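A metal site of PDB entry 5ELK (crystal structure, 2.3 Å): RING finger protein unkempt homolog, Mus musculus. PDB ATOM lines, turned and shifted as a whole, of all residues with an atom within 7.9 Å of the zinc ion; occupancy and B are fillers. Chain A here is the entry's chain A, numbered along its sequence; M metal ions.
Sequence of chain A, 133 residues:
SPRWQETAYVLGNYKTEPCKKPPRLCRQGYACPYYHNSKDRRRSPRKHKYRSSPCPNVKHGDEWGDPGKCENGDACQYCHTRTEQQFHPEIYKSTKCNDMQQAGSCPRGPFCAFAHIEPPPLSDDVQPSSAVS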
ATOM      1  N   ARG A  43      -4.661  13.428  -8.617  1.00  0.00           N
ATOM      2  CA  ARG A  43      -4.321  12.054  -8.945  1.00  0.00           C
ATOM      3  C   ARG A  43      -2.952  12.044  -9.622  1.00  0.00           C
ATOM      4  O   ARG A  43      -2.700  12.821 -10.545  1.00  0.00           O
ATOM      5  CB  ARG A  43      -5.383  11.437  -9.857  1.00  0.00           C
ATOM      6  CG  ARG A  43      -6.744  11.325  -9.197  1.00  0.00           C
ATOM      7  CD  ARG A  43      -7.845  11.063 -10.223  1.00  0.00           C
ATOM      8  NE  ARG A  43      -8.053  12.215 -11.088  1.00  0.00           N
ATOM      9  CZ  ARG A  43      -8.764  12.192 -12.214  1.00  0.00           C
ATOM     10  NH1 ARG A  43      -9.332  11.075 -12.626  1.00  0.00           N
ATOM     11  NH2 ARG A  43      -8.897  13.288 -12.928  1.00  0.00           N
ATOM     12  N   PRO A  54     -10.429  20.111 -18.587  1.00  0.00           N
ATOM     13  CA  PRO A  54     -11.288  19.997 -17.399  1.00  0.00           C
ATOM     14  C   PRO A  54     -12.489  19.066 -17.599  1.00  0.00           C
ATOM     15  O   PRO A  54     -13.032  19.030 -18.697  1.00  0.00           O
ATOM     16  CB  PRO A  54     -11.813  21.430 -17.202  1.00  0.00           C
ATOM     17  CG  PRO A  54     -10.907  22.298 -17.989  1.00  0.00           C
ATOM     18  CD  PRO A  54     -10.451  21.480 -19.139  1.00  0.00           C
ATOM     19  N   CYS A  55     -12.878  18.327 -16.554  1.00  0.00           N
ATOM     20  CA  CYS A  55     -14.124  17.574 -16.578  1.00  0.00           C
ATOM     21  C   CYS A  55     -15.283  18.553 -16.395  1.00  0.00           C
ATOM     22  O   CYS A  55     -15.342  19.256 -15.400  1.00  0.00           O
ATOM     23  CB  CYS A  55     -14.151  16.511 -15.476  1.00  0.00           C
ATOM     24  SG  CYS A  55     -15.660  15.478 -15.471  1.00  0.00           S
ATOM     25  N   PRO A  56     -16.203  18.610 -17.372  1.00  0.00           N
ATOM     26  CA  PRO A  56     -17.310  19.569 -17.272  1.00  0.00           C
ATOM     27  C   PRO A  56     -18.399  19.158 -16.284  1.00  0.00           C
ATOM     28  O   PRO A  56     -19.327  19.947 -16.043  1.00  0.00           O
ATOM     29  CB  PRO A  56     -17.845  19.627 -18.694  1.00  0.00           C
ATOM     30  CG  PRO A  56     -17.510  18.299 -19.246  1.00  0.00           C
ATOM     31  CD  PRO A  56     -16.213  17.898 -18.658  1.00  0.00           C
ATOM     32  N   ASN A  57     -18.280  17.971 -15.697  1.00  0.00           N
ATOM     33  CA  ASN A  57     -19.147  17.570 -14.587  1.00  0.00           C
ATOM     34  C   ASN A  57     -18.622  18.164 -13.291  1.00  0.00           C
ATOM     35  O   ASN A  57     -19.267  18.090 -12.264  1.00  0.00           O
ATOM     36  CB  ASN A  57     -19.239  16.047 -14.446  1.00  0.00           C
ATOM     37  CG  ASN A  57     -19.724  15.356 -15.709  1.00  0.00           C
ATOM     38  OD1 ASN A  57     -20.691  15.774 -16.331  1.00  0.00           O
ATOM     39  ND2 ASN A  57     -19.040  14.277 -16.092  1.00  0.00           N
ATOM     40  N   VAL A  58     -17.420  18.739 -13.339  1.00  0.00           N
ATOM     41  CA  VAL A  58     -16.817  19.329 -12.158  1.00  0.00           C
ATOM     42  C   VAL A  58     -16.596  20.808 -12.381  1.00  0.00           C
ATOM     43  O   VAL A  58     -16.936  21.618 -11.525  1.00  0.00           O
ATOM     44  CB  VAL A  58     -15.471  18.690 -11.827  1.00  0.00           C
ATOM     45  CG1 VAL A  58     -14.912  19.280 -10.517  1.00  0.00           C
ATOM     46  CG2 VAL A  58     -15.638  17.192 -11.738  1.00  0.00           C
ATOM     47  N   LYS A  59     -16.049  21.145 -13.529  1.00  0.00           N
ATOM     48  CA  LYS A  59     -15.804  22.543 -13.856  1.00  0.00           C
ATOM     49  C   LYS A  59     -16.937  23.080 -14.721  1.00  0.00           C
ATOM     50  O   LYS A  59     -17.017  22.794 -15.911  1.00  0.00           O
ATOM     51  CB  LYS A  59     -14.466  22.737 -14.554  1.00  0.00           C
ATOM     52  CG  LYS A  59     -14.101  24.203 -14.659  1.00  0.00           C
ATOM     53  CD  LYS A  59     -12.912  24.447 -15.544  1.00  0.00           C
ATOM     54  CE  LYS A  59     -12.406  25.879 -15.424  1.00  0.00           C
ATOM     55  NZ  LYS A  59     -11.176  26.102 -16.230  1.00  0.00           N
ATOM     56  N   PRO A  67     -15.318  17.583  -6.885  1.00  0.00           N
ATOM     57  CA  PRO A  67     -15.037  16.503  -7.847  1.00  0.00           C
ATOM     58  C   PRO A  67     -15.938  15.279  -7.697  1.00  0.00           C
ATOM     59  O   PRO A  67     -16.124  14.565  -8.682  1.00  0.00           O
ATOM     60  CB  PRO A  67     -13.578  16.139  -7.537  1.00  0.00           C
ATOM     61  CG  PRO A  67     -13.023  17.357  -6.901  1.00  0.00           C
ATOM     62  CD  PRO A  67     -14.132  17.856  -6.058  1.00  0.00           C
ATOM     63  N   LYS A  69     -19.665  14.056  -7.651  1.00  0.00           N
ATOM     64  CA  LYS A  69     -20.669  14.597  -8.586  1.00  0.00           C
ATOM     65  C   LYS A  69     -20.174  14.473 -10.009  1.00  0.00           C
ATOM     66  O   LYS A  69     -20.862  14.857 -10.945  1.00  0.00           O
ATOM     67  CB  LYS A  69     -21.086  16.053  -8.292  1.00  0.00           C
ATOM     68  CG  LYS A  69     -21.552  16.291  -6.858  1.00  0.00           C
ATOM     69  CD  LYS A  69     -21.987  17.739  -6.615  1.00  0.00           C
ATOM     70  CE  LYS A  69     -22.810  17.850  -5.333  1.00  0.00           C
ATOM     71  NZ  LYS A  69     -24.109  17.124  -5.429  1.00  0.00           N
ATOM     72  N   CYS A  70     -18.959  13.956 -10.162  1.00  0.00           N
ATOM     73  CA  CYS A  70     -18.624  13.249 -11.376  1.00  0.00           C
ATOM     74  C   CYS A  70     -18.737  11.768 -11.071  1.00  0.00           C
ATOM     75  O   CYS A  70     -18.009  11.244 -10.237  1.00  0.00           O
ATOM     76  CB  CYS A  70     -17.242  13.565 -11.909  1.00  0.00           C
ATOM     77  SG  CYS A  70     -16.946  12.649 -13.433  1.00  0.00           S
ATOM     78  N   GLU A  71     -19.678  11.113 -11.740  1.00  0.00           N
ATOM     79  CA  GLU A  71     -20.000   9.722 -11.482  1.00  0.00           C
ATOM     80  C   GLU A  71     -18.884   8.776 -11.921  1.00  0.00           C
ATOM     81  O   GLU A  71     -18.920   7.580 -11.623  1.00  0.00           O
ATOM     82  CB  GLU A  71     -21.287   9.403 -12.228  1.00  0.00           C
ATOM     83  CG  GLU A  71     -22.472  10.227 -11.762  1.00  0.00           C
ATOM     84  CD  GLU A  71     -23.015   9.792 -10.421  1.00  0.00           C
ATOM     85  OE1 GLU A  71     -22.745   8.640 -10.000  1.00  0.00           O
ATOM     86  OE2 GLU A  71     -23.701  10.610  -9.773  1.00  0.00           O
ATOM     87  N   ASN A  72     -17.898   9.320 -12.628  1.00  0.00           N
ATOM     88  CA  ASN A  72     -16.785   8.513 -13.135  1.00  0.00           C
ATOM     89  C   ASN A  72     -15.765   8.214 -12.040  1.00  0.00           C
ATOM     90  O   ASN A  72     -15.099   7.190 -12.066  1.00  0.00           O
ATOM     91  CB  ASN A  72     -16.109   9.244 -14.295  1.00  0.00           C
ATOM     92  CG  ASN A  72     -16.931   9.208 -15.563  1.00  0.00           C
ATOM     93  OD1 ASN A  72     -17.543   8.191 -15.896  1.00  0.00           O
ATOM     94  ND2 ASN A  72     -16.946  10.331 -16.281  1.00  0.00           N
ATOM     95  N   GLY A  73     -15.676   9.109 -11.058  1.00  0.00           N
ATOM     96  CA  GLY A  73     -14.717   8.957  -9.987  1.00  0.00           C
ATOM     97  C   GLY A  73     -13.297   9.128 -10.499  1.00  0.00           C
ATOM     98  O   GLY A  73     -13.052   9.822 -11.479  1.00  0.00           O
ATOM     99  N   ASP A  74     -12.348   8.469  -9.833  1.00  0.00           N
ATOM    100  CA  ASP A  74     -10.933   8.619 -10.137  1.00  0.00           C
ATOM    101  C   ASP A  74     -10.524   7.972 -11.467  1.00  0.00           C
ATOM    102  O   ASP A  74      -9.353   8.007 -11.834  1.00  0.00           O
ATOM    103  CB  ASP A  74     -10.098   8.034  -8.995  1.00  0.00           C
ATOM    104  CG  ASP A  74     -10.071   8.939  -7.765  1.00  0.00           C
ATOM    105  OD1 ASP A  74     -10.405  10.134  -7.883  1.00  0.00           O
ATOM    106  OD2 ASP A  74      -9.683   8.440  -6.692  1.00  0.00           O
ATOM    107  N   ALA A  75     -11.482   7.409 -12.186  1.00  0.00           N
ATOM    108  CA  ALA A  75     -11.207   6.794 -13.474  1.00  0.00           C
ATOM    109  C   ALA A  75     -11.525   7.750 -14.608  1.00  0.00           C
ATOM    110  O   ALA A  75     -11.366   7.410 -15.785  1.00  0.00           O
ATOM    111  CB  ALA A  75     -12.014   5.515 -13.631  1.00  0.00           C
ATOM    112  N   CYS A  76     -11.966   8.952 -14.267  1.00  0.00           N
ATOM    113  CA  CYS A  76     -12.267   9.966 -15.278  1.00  0.00           C
ATOM    114  C   CYS A  76     -11.013  10.389 -16.028  1.00  0.00           C
ATOM    115  O   CYS A  76      -9.972  10.626 -15.433  1.00  0.00           O
ATOM    116  CB  CYS A  76     -12.940  11.192 -14.656  1.00  0.00           C
ATOM    117  SG  CYS A  76     -13.879  12.160 -15.872  1.00  0.00           S
ATOM    118  N   GLN A  77     -11.138  10.473 -17.355  1.00  0.00           N
ATOM    119  CA  GLN A  77     -10.020  10.812 -18.224  1.00  0.00           C
ATOM    120  C   GLN A  77      -9.954  12.322 -18.467  1.00  0.00           C
ATOM    121  O   GLN A  77      -9.470  12.782 -19.502  1.00  0.00           O
ATOM    122  CB  GLN A  77     -10.164  10.060 -19.545  1.00  0.00           C
ATOM    123  CG  GLN A  77     -10.147   8.559 -19.368  1.00  0.00           C
ATOM    124  CD  GLN A  77      -8.759   7.991 -19.475  1.00  0.00           C
ATOM    125  OE1 GLN A  77      -8.168   7.986 -20.554  1.00  0.00           O
ATOM    126  NE2 GLN A  77      -8.223   7.497 -18.358  1.00  0.00           N
ATOM    127  N   TYR A  78     -10.454  13.071 -17.493  1.00  0.00           N
ATOM    128  CA  TYR A  78     -10.451  14.521 -17.546  1.00  0.00           C
ATOM    129  C   TYR A  78      -9.974  15.020 -16.196  1.00  0.00           C
ATOM    130  O   TYR A  78     -10.038  14.281 -15.211  1.00  0.00           O
ATOM    131  CB  TYR A  78     -11.862  15.027 -17.807  1.00  0.00           C
ATOM    132  CG  TYR A  78     -12.365  14.749 -19.213  1.00  0.00           C
ATOM    133  CD1 TYR A  78     -12.934  13.527 -19.553  1.00  0.00           C
ATOM    134  CD2 TYR A  78     -12.280  15.720 -20.189  1.00  0.00           C
ATOM    135  CE1 TYR A  78     -13.399  13.282 -20.828  1.00  0.00           C
ATOM    136  CE2 TYR A  78     -12.748  15.483 -21.476  1.00  0.00           C
ATOM    137  CZ  TYR A  78     -13.306  14.262 -21.785  1.00  0.00           C
ATOM    138  OH  TYR A  78     -13.762  14.021 -23.060  1.00  0.00           O
ATOM    139  N   CYS A  79      -9.510  16.267 -16.136  1.00  0.00           N
ATOM    140  CA  CYS A  79      -9.060  16.833 -14.873  1.00  0.00           C
ATOM    141  C   CYS A  79     -10.225  17.153 -13.940  1.00  0.00           C
ATOM    142  O   CYS A  79     -11.267  17.613 -14.392  1.00  0.00           O
ATOM    143  CB  CYS A  79      -8.241  18.100 -15.120  1.00  0.00           C
ATOM    144  SG  CYS A  79      -6.668  17.787 -15.944  1.00  0.00           S
ATOM    145  N   HIS A  80     -10.025  16.915 -12.648  1.00  0.00           N
ATOM    146  CA  HIS A  80     -11.045  17.116 -11.627  1.00  0.00           C
ATOM    147  C   HIS A  80     -10.714  18.263 -10.661  1.00  0.00           C
ATOM    148  O   HIS A  80     -11.548  18.649  -9.842  1.00  0.00           O
ATOM    149  CB  HIS A  80     -11.257  15.830 -10.827  1.00  0.00           C
ATOM    150  CG  HIS A  80     -12.211  14.868 -11.459  1.00  0.00           C
ATOM    151  ND1 HIS A  80     -12.449  13.603 -10.952  1.00  0.00           N
ATOM    152  CD2 HIS A  80     -12.989  14.976 -12.566  1.00  0.00           C
ATOM    153  CE1 HIS A  80     -13.315  12.978 -11.722  1.00  0.00           C
ATOM    154  NE2 HIS A  80     -13.662  13.790 -12.708  1.00  0.00           N
HETATM  155 ZN    ZN M   1     -14.895  13.503 -14.324  1.00  0.00          ZN
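SG of Cys 76 lies close to ND2 of Asn 72 (3.6 Å).
The side-chain sulfur (SG) of Cys 70 sits close to the side-chain amide nitrogen (ND2) of Asn 57 (3.8 Å).
SG of Cys 55 sits close to N of Asn 57, at 3.6 Å.
O of Cys 76 is in hydrogen-bond range of NH1 of Arg 43.
N of Cys 55 lies within hydrogen-bond range of O of Cys 79 (2.8 Å).
N of Asn 72 sits close to SG of Cys 70.
The zinc ion is bound by a ring nitrogen (NE2) of His 80 (2.1 Å), the side-chain sulfur of Cys 76 (2.3 Å), the side-chain sulfur of Cys 70 (2.4 Å) and the side-chain sulfur of Cys 55 (2.4 Å).
The nearest printed residue that does not touch the zinc ion is Asn 72 (4.3 Å).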
